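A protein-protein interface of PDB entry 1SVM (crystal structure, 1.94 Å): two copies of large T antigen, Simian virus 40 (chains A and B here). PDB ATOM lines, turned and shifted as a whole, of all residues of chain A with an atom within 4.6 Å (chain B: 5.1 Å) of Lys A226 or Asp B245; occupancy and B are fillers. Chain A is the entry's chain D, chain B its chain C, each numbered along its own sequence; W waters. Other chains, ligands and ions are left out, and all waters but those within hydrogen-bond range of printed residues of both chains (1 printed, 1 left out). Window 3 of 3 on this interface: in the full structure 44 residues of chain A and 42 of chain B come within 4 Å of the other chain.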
ATOM      1  N   ASN A 201     -27.031 -15.141  -6.403  1.00  0.00           N
ATOM      2  CA  ASN A 201     -25.745 -15.305  -5.728  1.00  0.00           C
ATOM      3  C   ASN A 201     -25.551 -14.197  -4.697  1.00  0.00           C
ATOM      4  O   ASN A 201     -24.616 -14.234  -3.902  1.00  0.00           O
ATOM      5  CB  ASN A 201     -24.591 -15.276  -6.736  1.00  0.00           C
ATOM      6  CG  ASN A 201     -24.618 -16.460  -7.677  1.00  0.00           C
ATOM      7  OD1 ASN A 201     -24.694 -17.608  -7.243  1.00  0.00           O
ATOM      8  ND2 ASN A 201     -24.553 -16.189  -8.972  1.00  0.00           N
ATOM      9  N   ASP A 224     -25.265 -18.301 -13.824  1.00  0.00           N
ATOM     10  CA  ASP A 224     -24.062 -18.618 -13.065  1.00  0.00           C
ATOM     11  C   ASP A 224     -24.267 -18.815 -11.568  1.00  0.00           C
ATOM     12  O   ASP A 224     -23.738 -18.058 -10.753  1.00  0.00           O
ATOM     13  CB  ASP A 224     -23.021 -17.522 -13.311  1.00  0.00           C
ATOM     14  CG  ASP A 224     -21.728 -18.066 -13.885  1.00  0.00           C
ATOM     15  OD1 ASP A 224     -20.942 -17.272 -14.446  1.00  0.00           O
ATOM     16  OD2 ASP A 224     -21.492 -19.288 -13.772  1.00  0.00           O
ATOM     17  N   VAL A 225     -25.025 -19.845 -11.213  1.00  0.00           N
ATOM     18  CA  VAL A 225     -25.304 -20.156  -9.820  1.00  0.00           C
ATOM     19  C   VAL A 225     -24.123 -20.919  -9.229  1.00  0.00           C
ATOM     20  O   VAL A 225     -23.679 -21.915  -9.796  1.00  0.00           O
ATOM     21  CB  VAL A 225     -26.579 -21.027  -9.705  1.00  0.00           C
ATOM     22  CG1 VAL A 225     -26.898 -21.298  -8.254  1.00  0.00           C
ATOM     23  CG2 VAL A 225     -27.750 -20.329 -10.400  1.00  0.00           C
ATOM     24  N   LYS A 226     -23.612 -20.451  -8.094  1.00  0.00           N
ATOM     25  CA  LYS A 226     -22.480 -21.109  -7.451  1.00  0.00           C
ATOM     26  C   LYS A 226     -22.872 -22.054  -6.323  1.00  0.00           C
ATOM     27  O   LYS A 226     -23.838 -21.813  -5.597  1.00  0.00           O
ATOM     28  CB  LYS A 226     -21.491 -20.071  -6.917  1.00  0.00           C
ATOM     29  CG  LYS A 226     -20.639 -19.423  -7.988  1.00  0.00           C
ATOM     30  CD  LYS A 226     -19.444 -18.697  -7.382  1.00  0.00           C
ATOM     31  CE  LYS A 226     -19.859 -17.421  -6.685  1.00  0.00           C
ATOM     32  NZ  LYS A 226     -20.560 -16.536  -7.648  1.00  0.00           N
ATOM     33  N   GLY A 227     -22.105 -23.133  -6.193  1.00  0.00           N
ATOM     34  CA  GLY A 227     -22.342 -24.120  -5.155  1.00  0.00           C
ATOM     35  C   GLY A 227     -21.230 -24.094  -4.120  1.00  0.00           C
ATOM     36  O   GLY A 227     -20.453 -23.144  -4.068  1.00  0.00           O
ATOM     37  N   PRO A 236     -14.852 -21.007  -6.940  1.00  0.00           N
ATOM     38  CA  PRO A 236     -15.214 -20.319  -5.698  1.00  0.00           C
ATOM     39  C   PRO A 236     -16.521 -20.859  -5.136  1.00  0.00           C
ATOM     40  O   PRO A 236     -17.330 -21.433  -5.863  1.00  0.00           O
ATOM     41  CB  PRO A 236     -15.333 -18.860  -6.132  1.00  0.00           C
ATOM     42  CG  PRO A 236     -14.386 -18.771  -7.296  1.00  0.00           C
ATOM     43  CD  PRO A 236     -14.690 -20.045  -8.043  1.00  0.00           C
ATOM     44  N   SER A 237     -16.725 -20.683  -3.840  1.00  0.00           N
ATOM     45  CA  SER A 237     -17.953 -21.157  -3.224  1.00  0.00           C
ATOM     46  C   SER A 237     -18.971 -20.031  -3.123  1.00  0.00           C
ATOM     47  O   SER A 237     -18.610 -18.858  -3.029  1.00  0.00           O
ATOM     48  CB  SER A 237     -17.661 -21.741  -1.843  1.00  0.00           C
ATOM     49  OG  SER A 237     -16.928 -22.947  -1.965  1.00  0.00           O
ATOM     50  N   GLY A 238     -20.247 -20.400  -3.160  1.00  0.00           N
ATOM     51  CA  GLY A 238     -21.314 -19.423  -3.072  1.00  0.00           C
ATOM     52  C   GLY A 238     -22.567 -20.076  -2.522  1.00  0.00           C
ATOM     53  O   GLY A 238     -22.584 -21.284  -2.289  1.00  0.00           O
ATOM     54  N   GLN A 239     -23.616 -19.283  -2.323  1.00  0.00           N
ATOM     55  CA  GLN A 239     -24.871 -19.793  -1.787  1.00  0.00           C
ATOM     56  C   GLN A 239     -25.948 -19.998  -2.848  1.00  0.00           C
ATOM     57  O   GLN A 239     -27.058 -20.429  -2.531  1.00  0.00           O
ATOM     58  CB  GLN A 239     -25.399 -18.840  -0.713  1.00  0.00           C
ATOM     59  CG  GLN A 239     -24.541 -18.791   0.539  1.00  0.00           C
ATOM     60  CD  GLN A 239     -24.335 -20.164   1.149  1.00  0.00           C
ATOM     61  OE1 GLN A 239     -25.296 -20.870   1.462  1.00  0.00           O
ATOM     62  NE2 GLN A 239     -23.076 -20.551   1.321  1.00  0.00           N
ATOM     63  N   GLY A 240     -25.618 -19.691  -4.099  1.00  0.00           N
ATOM     64  CA  GLY A 240     -26.573 -19.839  -5.184  1.00  0.00           C
ATOM     65  C   GLY A 240     -27.345 -21.147  -5.180  1.00  0.00           C
ATOM     66  O   GLY A 240     -28.577 -21.155  -5.201  1.00  0.00           O
ATOM     67  N   ILE A 241     -26.623 -22.263  -5.154  1.00  0.00           N
ATOM     68  CA  ILE A 241     -27.256 -23.575  -5.155  1.00  0.00           C
ATOM     69  C   ILE A 241     -28.110 -23.795  -3.908  1.00  0.00           C
ATOM     70  O   ILE A 241     -29.228 -24.295  -4.002  1.00  0.00           O
ATOM     71  CB  ILE A 241     -26.199 -24.689  -5.272  1.00  0.00           C
ATOM     72  CG1 ILE A 241     -25.477 -24.564  -6.614  1.00  0.00           C
ATOM     73  CG2 ILE A 241     -26.850 -26.051  -5.136  1.00  0.00           C
ATOM     74  CD1 ILE A 241     -26.404 -24.613  -7.809  1.00  0.00           C
ATOM     75  N   TYR A 281     -20.681 -27.693 -10.284  1.00  0.00           N
ATOM     76  CA  TYR A 281     -20.616 -27.810  -8.833  1.00  0.00           C
ATOM     77  C   TYR A 281     -21.458 -29.041  -8.533  1.00  0.00           C
ATOM     78  O   TYR A 281     -22.117 -29.575  -9.430  1.00  0.00           O
ATOM     79  CB  TYR A 281     -21.252 -26.600  -8.134  1.00  0.00           C
ATOM     80  CG  TYR A 281     -20.449 -25.316  -8.171  1.00  0.00           C
ATOM     81  CD1 TYR A 281     -20.540 -24.440  -9.252  1.00  0.00           C
ATOM     82  CD2 TYR A 281     -19.617 -24.963  -7.106  1.00  0.00           C
ATOM     83  CE1 TYR A 281     -19.827 -23.241  -9.271  1.00  0.00           C
ATOM     84  CE2 TYR A 281     -18.898 -23.772  -7.115  1.00  0.00           C
ATOM     85  CZ  TYR A 281     -19.007 -22.915  -8.198  1.00  0.00           C
ATOM     86  OH  TYR A 281     -18.302 -21.729  -8.209  1.00  0.00           O
ATOM     87  N   ILE B 241     -13.643  -8.707  -3.787  1.00  0.00           N
ATOM     88  CA  ILE B 241     -13.402  -9.689  -4.835  1.00  0.00           C
ATOM     89  C   ILE B 241     -14.498 -10.747  -4.857  1.00  0.00           C
ATOM     90  O   ILE B 241     -14.999 -11.098  -5.927  1.00  0.00           O
ATOM     91  CB  ILE B 241     -12.020 -10.354  -4.668  1.00  0.00           C
ATOM     92  CG1 ILE B 241     -10.926  -9.323  -4.961  1.00  0.00           C
ATOM     93  CG2 ILE B 241     -11.881 -11.550  -5.610  1.00  0.00           C
ATOM     94  CD1 ILE B 241     -10.998  -8.729  -6.363  1.00  0.00           C
ATOM     95  N   ASN B 242     -14.879 -11.245  -3.683  1.00  0.00           N
ATOM     96  CA  ASN B 242     -15.937 -12.246  -3.602  1.00  0.00           C
ATOM     97  C   ASN B 242     -17.230 -11.666  -4.162  1.00  0.00           C
ATOM     98  O   ASN B 242     -17.995 -12.360  -4.838  1.00  0.00           O
ATOM     99  CB  ASN B 242     -16.171 -12.689  -2.153  1.00  0.00           C
ATOM    100  CG  ASN B 242     -14.991 -13.449  -1.573  1.00  0.00           C
ATOM    101  OD1 ASN B 242     -14.378 -14.281  -2.249  1.00  0.00           O
ATOM    102  ND2 ASN B 242     -14.679 -13.181  -0.311  1.00  0.00           N
ATOM    103  N   ASN B 243     -17.473 -10.391  -3.884  1.00  0.00           N
ATOM    104  CA  ASN B 243     -18.681  -9.742  -4.381  1.00  0.00           C
ATOM    105  C   ASN B 243     -18.682  -9.665  -5.902  1.00  0.00           C
ATOM    106  O   ASN B 243     -19.692  -9.973  -6.541  1.00  0.00           O
ATOM    107  CB  ASN B 243     -18.827  -8.341  -3.781  1.00  0.00           C
ATOM    108  CG  ASN B 243     -19.164  -8.377  -2.294  1.00  0.00           C
ATOM    109  OD1 ASN B 243     -19.512  -9.427  -1.746  1.00  0.00           O
ATOM    110  ND2 ASN B 243     -19.070  -7.224  -1.641  1.00  0.00           N
ATOM    111  N   LEU B 244     -17.560  -9.260  -6.490  1.00  0.00           N
ATOM    112  CA  LEU B 244     -17.481  -9.178  -7.943  1.00  0.00           C
ATOM    113  C   LEU B 244     -17.686 -10.554  -8.564  1.00  0.00           C
ATOM    114  O   LEU B 244     -18.294 -10.679  -9.626  1.00  0.00           O
ATOM    115  CB  LEU B 244     -16.126  -8.614  -8.396  1.00  0.00           C
ATOM    116  CG  LEU B 244     -15.914  -7.102  -8.272  1.00  0.00           C
ATOM    117  CD1 LEU B 244     -14.566  -6.726  -8.878  1.00  0.00           C
ATOM    118  CD2 LEU B 244     -17.038  -6.372  -8.995  1.00  0.00           C
ATOM    119  N   ASP B 245     -17.182 -11.592  -7.906  1.00  0.00           N
ATOM    120  CA  ASP B 245     -17.340 -12.934  -8.446  1.00  0.00           C
ATOM    121  C   ASP B 245     -18.793 -13.408  -8.372  1.00  0.00           C
ATOM    122  O   ASP B 245     -19.147 -14.426  -8.972  1.00  0.00           O
ATOM    123  CB  ASP B 245     -16.434 -13.930  -7.719  1.00  0.00           C
ATOM    124  CG  ASP B 245     -16.338 -15.259  -8.451  1.00  0.00           C
ATOM    125  OD1 ASP B 245     -16.857 -16.268  -7.930  1.00  0.00           O
ATOM    126  OD2 ASP B 245     -15.754 -15.287  -9.557  1.00  0.00           O
ATOM    127  N   ASN B 246     -19.626 -12.685  -7.623  1.00  0.00           N
ATOM    128  CA  ASN B 246     -21.046 -13.027  -7.522  1.00  0.00           C
ATOM    129  C   ASN B 246     -21.838 -12.193  -8.528  1.00  0.00           C
ATOM    130  O   ASN B 246     -23.055 -12.340  -8.650  1.00  0.00           O
ATOM    131  CB  ASN B 246     -21.587 -12.762  -6.107  1.00  0.00           C
ATOM    132  CG  ASN B 246     -21.185 -13.842  -5.114  1.00  0.00           C
ATOM    133  OD1 ASN B 246     -21.199 -15.025  -5.436  1.00  0.00           O
ATOM    134  ND2 ASN B 246     -20.845 -13.436  -3.898  1.00  0.00           N
ATOM    135  N   LEU B 247     -21.129 -11.329  -9.250  1.00  0.00           N
ATOM    136  CA  LEU B 247     -21.730 -10.445 -10.248  1.00  0.00           C
ATOM    137  C   LEU B 247     -21.231 -10.754 -11.661  1.00  0.00           C
ATOM    138  O   LEU B 247     -21.090  -9.857 -12.494  1.00  0.00           O
ATOM    139  CB  LEU B 247     -21.416  -8.984  -9.901  1.00  0.00           C
ATOM    140  CG  LEU B 247     -21.958  -8.460  -8.567  1.00  0.00           C
ATOM    141  CD1 LEU B 247     -21.412  -7.062  -8.295  1.00  0.00           C
ATOM    142  CD2 LEU B 247     -23.489  -8.439  -8.608  1.00  0.00           C
ATOM    143  N   ARG B 248     -20.978 -12.028 -11.932  1.00  0.00           N
ATOM    144  CA  ARG B 248     -20.489 -12.441 -13.239  1.00  0.00           C
ATOM    145  C   ARG B 248     -21.395 -12.003 -14.389  1.00  0.00           C
ATOM    146  O   ARG B 248     -20.904 -11.687 -15.474  1.00  0.00           O
ATOM    147  CB  ARG B 248     -20.308 -13.958 -13.274  1.00  0.00           C
ATOM    148  CG  ARG B 248     -19.357 -14.485 -12.207  1.00  0.00           C
ATOM    149  CD  ARG B 248     -19.354 -16.011 -12.185  1.00  0.00           C
ATOM    150  NE  ARG B 248     -18.580 -16.534 -11.064  1.00  0.00           N
ATOM    151  CZ  ARG B 248     -18.483 -17.823 -10.757  1.00  0.00           C
ATOM    152  NH1 ARG B 248     -19.109 -18.731 -11.492  1.00  0.00           N
ATOM    153  NH2 ARG B 248     -17.765 -18.201  -9.707  1.00  0.00           N
ATOM    154  N   PRO B 284      -9.683 -15.013  -8.524  1.00  0.00           N
ATOM    155  CA  PRO B 284     -10.184 -16.331  -8.923  1.00  0.00           C
ATOM    156  C   PRO B 284     -10.321 -16.437 -10.440  1.00  0.00           C
ATOM    157  O   PRO B 284     -10.660 -15.463 -11.112  1.00  0.00           O
ATOM    158  CB  PRO B 284     -11.539 -16.419  -8.214  1.00  0.00           C
ATOM    159  CG  PRO B 284     -11.366 -15.531  -7.027  1.00  0.00           C
ATOM    160  CD  PRO B 284     -10.627 -14.352  -7.609  1.00  0.00           C
ATOM    161  N   THR B 286     -12.552 -17.709 -12.332  1.00  0.00           N
ATOM    162  CA  THR B 286     -13.865 -17.340 -12.847  1.00  0.00           C
ATOM    163  C   THR B 286     -13.974 -15.837 -13.093  1.00  0.00           C
ATOM    164  O   THR B 286     -14.566 -15.401 -14.079  1.00  0.00           O
ATOM    165  CB  THR B 286     -14.966 -17.776 -11.871  1.00  0.00           C
ATOM    166  OG1 THR B 286     -14.609 -17.374 -10.546  1.00  0.00           O
ATOM    167  CG2 THR B 286     -15.143 -19.292 -11.906  1.00  0.00           C
ATOM    168  N   LEU B 287     -13.390 -15.049 -12.196  1.00  0.00           N
ATOM    169  CA  LEU B 287     -13.420 -13.599 -12.317  1.00  0.00           C
ATOM    170  C   LEU B 287     -12.413 -13.124 -13.366  1.00  0.00           C
ATOM    171  O   LEU B 287     -12.724 -12.266 -14.195  1.00  0.00           O
ATOM    172  CB  LEU B 287     -13.116 -12.954 -10.960  1.00  0.00           C
ATOM    173  CG  LEU B 287     -13.169 -11.425 -10.880  1.00  0.00           C
ATOM    174  CD1 LEU B 287     -14.534 -10.927 -11.343  1.00  0.00           C
ATOM    175  CD2 LEU B 287     -12.899 -10.989  -9.443  1.00  0.00           C
HETATM  176  O   HOH W   1     -22.608 -16.675  -3.818  1.00  0.00           O
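The side-chain carboxylate of Asp B245 lies within salt-bridge range of the guanidinium group of Arg B248, 2.8 Å away.
ND2 of Asn A201 sits at hydrogen-bond distance from O of Asp A224.
OD1 of Asn A201 lies within hydrogen-bond range of N of Lys A226, 3.2 Å away.
The backbone carbonyl oxygen (O) of Lys A226 is in hydrogen-bond range of the backbone NH (N) of Gly A240 (3.1 Å).
O of Lys A226 lies within hydrogen-bond range of N of Ile A241.
O of Pro A236 lies within hydrogen-bond range of OH of Tyr A281.
OD1 of Asp B245 is in salt-bridge range of NZ of Lys A226, 3.7 Å away.
The side-chain amide oxygen of Asn B246 sits at hydrogen-bond distance from the side-chain amino group of Lys A226.
OD2 of Asp A224 lies within salt-bridge range of NH1 of Arg B248 (3.3 Å).
Asn A201 touches Asn B246.
CD of Lys A226 touches NH2 of Arg B248 (2.9 Å).
CB of Pro A236 touches OD1 of Asp B245, 3.5 Å away.
Pro A236 touches Arg B248 (CD to NH2, 3.95 Å).
Pro A236 touches Pro B284 (CG to CB, 3.8 Å).
OG1 of Thr B286 touches CG of Pro A236, at 3.5 Å.
NH2 of Arg B248 touches OH of Tyr A281, 3.9 Å away.
Lys A226 touches three residues of chain B.
Asp B245 touches two residues of chain A.
Of the printed residues of chain B, Pro A236 touches Asp B245 (3.5 Å), Arg B248 (3.95 Å), Pro B284 (3.8 Å) and Thr B286 (3.5 Å).
Of the printed residues of chain B, Asn A201 touches Asn B246 (3.6 Å).
Printed residues of chain A within 4 Å of Arg B248: Asp A224, Lys A226, Pro A236 and Tyr A281.
Ile A241 touches none of the printed residues of chain B.
The nearest printed residue of chain B that does not touch Lys A226 is Leu B247 (5.5 Å).
Printed residues of chain B that touch a printed residue of chain A: Asp B245, Asn B246, Arg B248, Pro B284 and Thr B286.
Hydrophobic or aromatic side chains of chain B that line the printed part of chain A: Pro B284.
Among the printed residues, Asp or Glu carboxylates within 4 Å of a Lys or Arg side-chain nitrogen of the other chain: Asp A224 with Arg B248 (3.3 Å) and Lys A226 with Asp B245 (3.7 Å).
Water W1 lies within hydrogen-bond range of OD1 of Asn B246 (2.7 Å), O of Asn A201 (3.2 Å) and N of Gln A239 (3.2 Å).
Position printed for both chains: 241.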
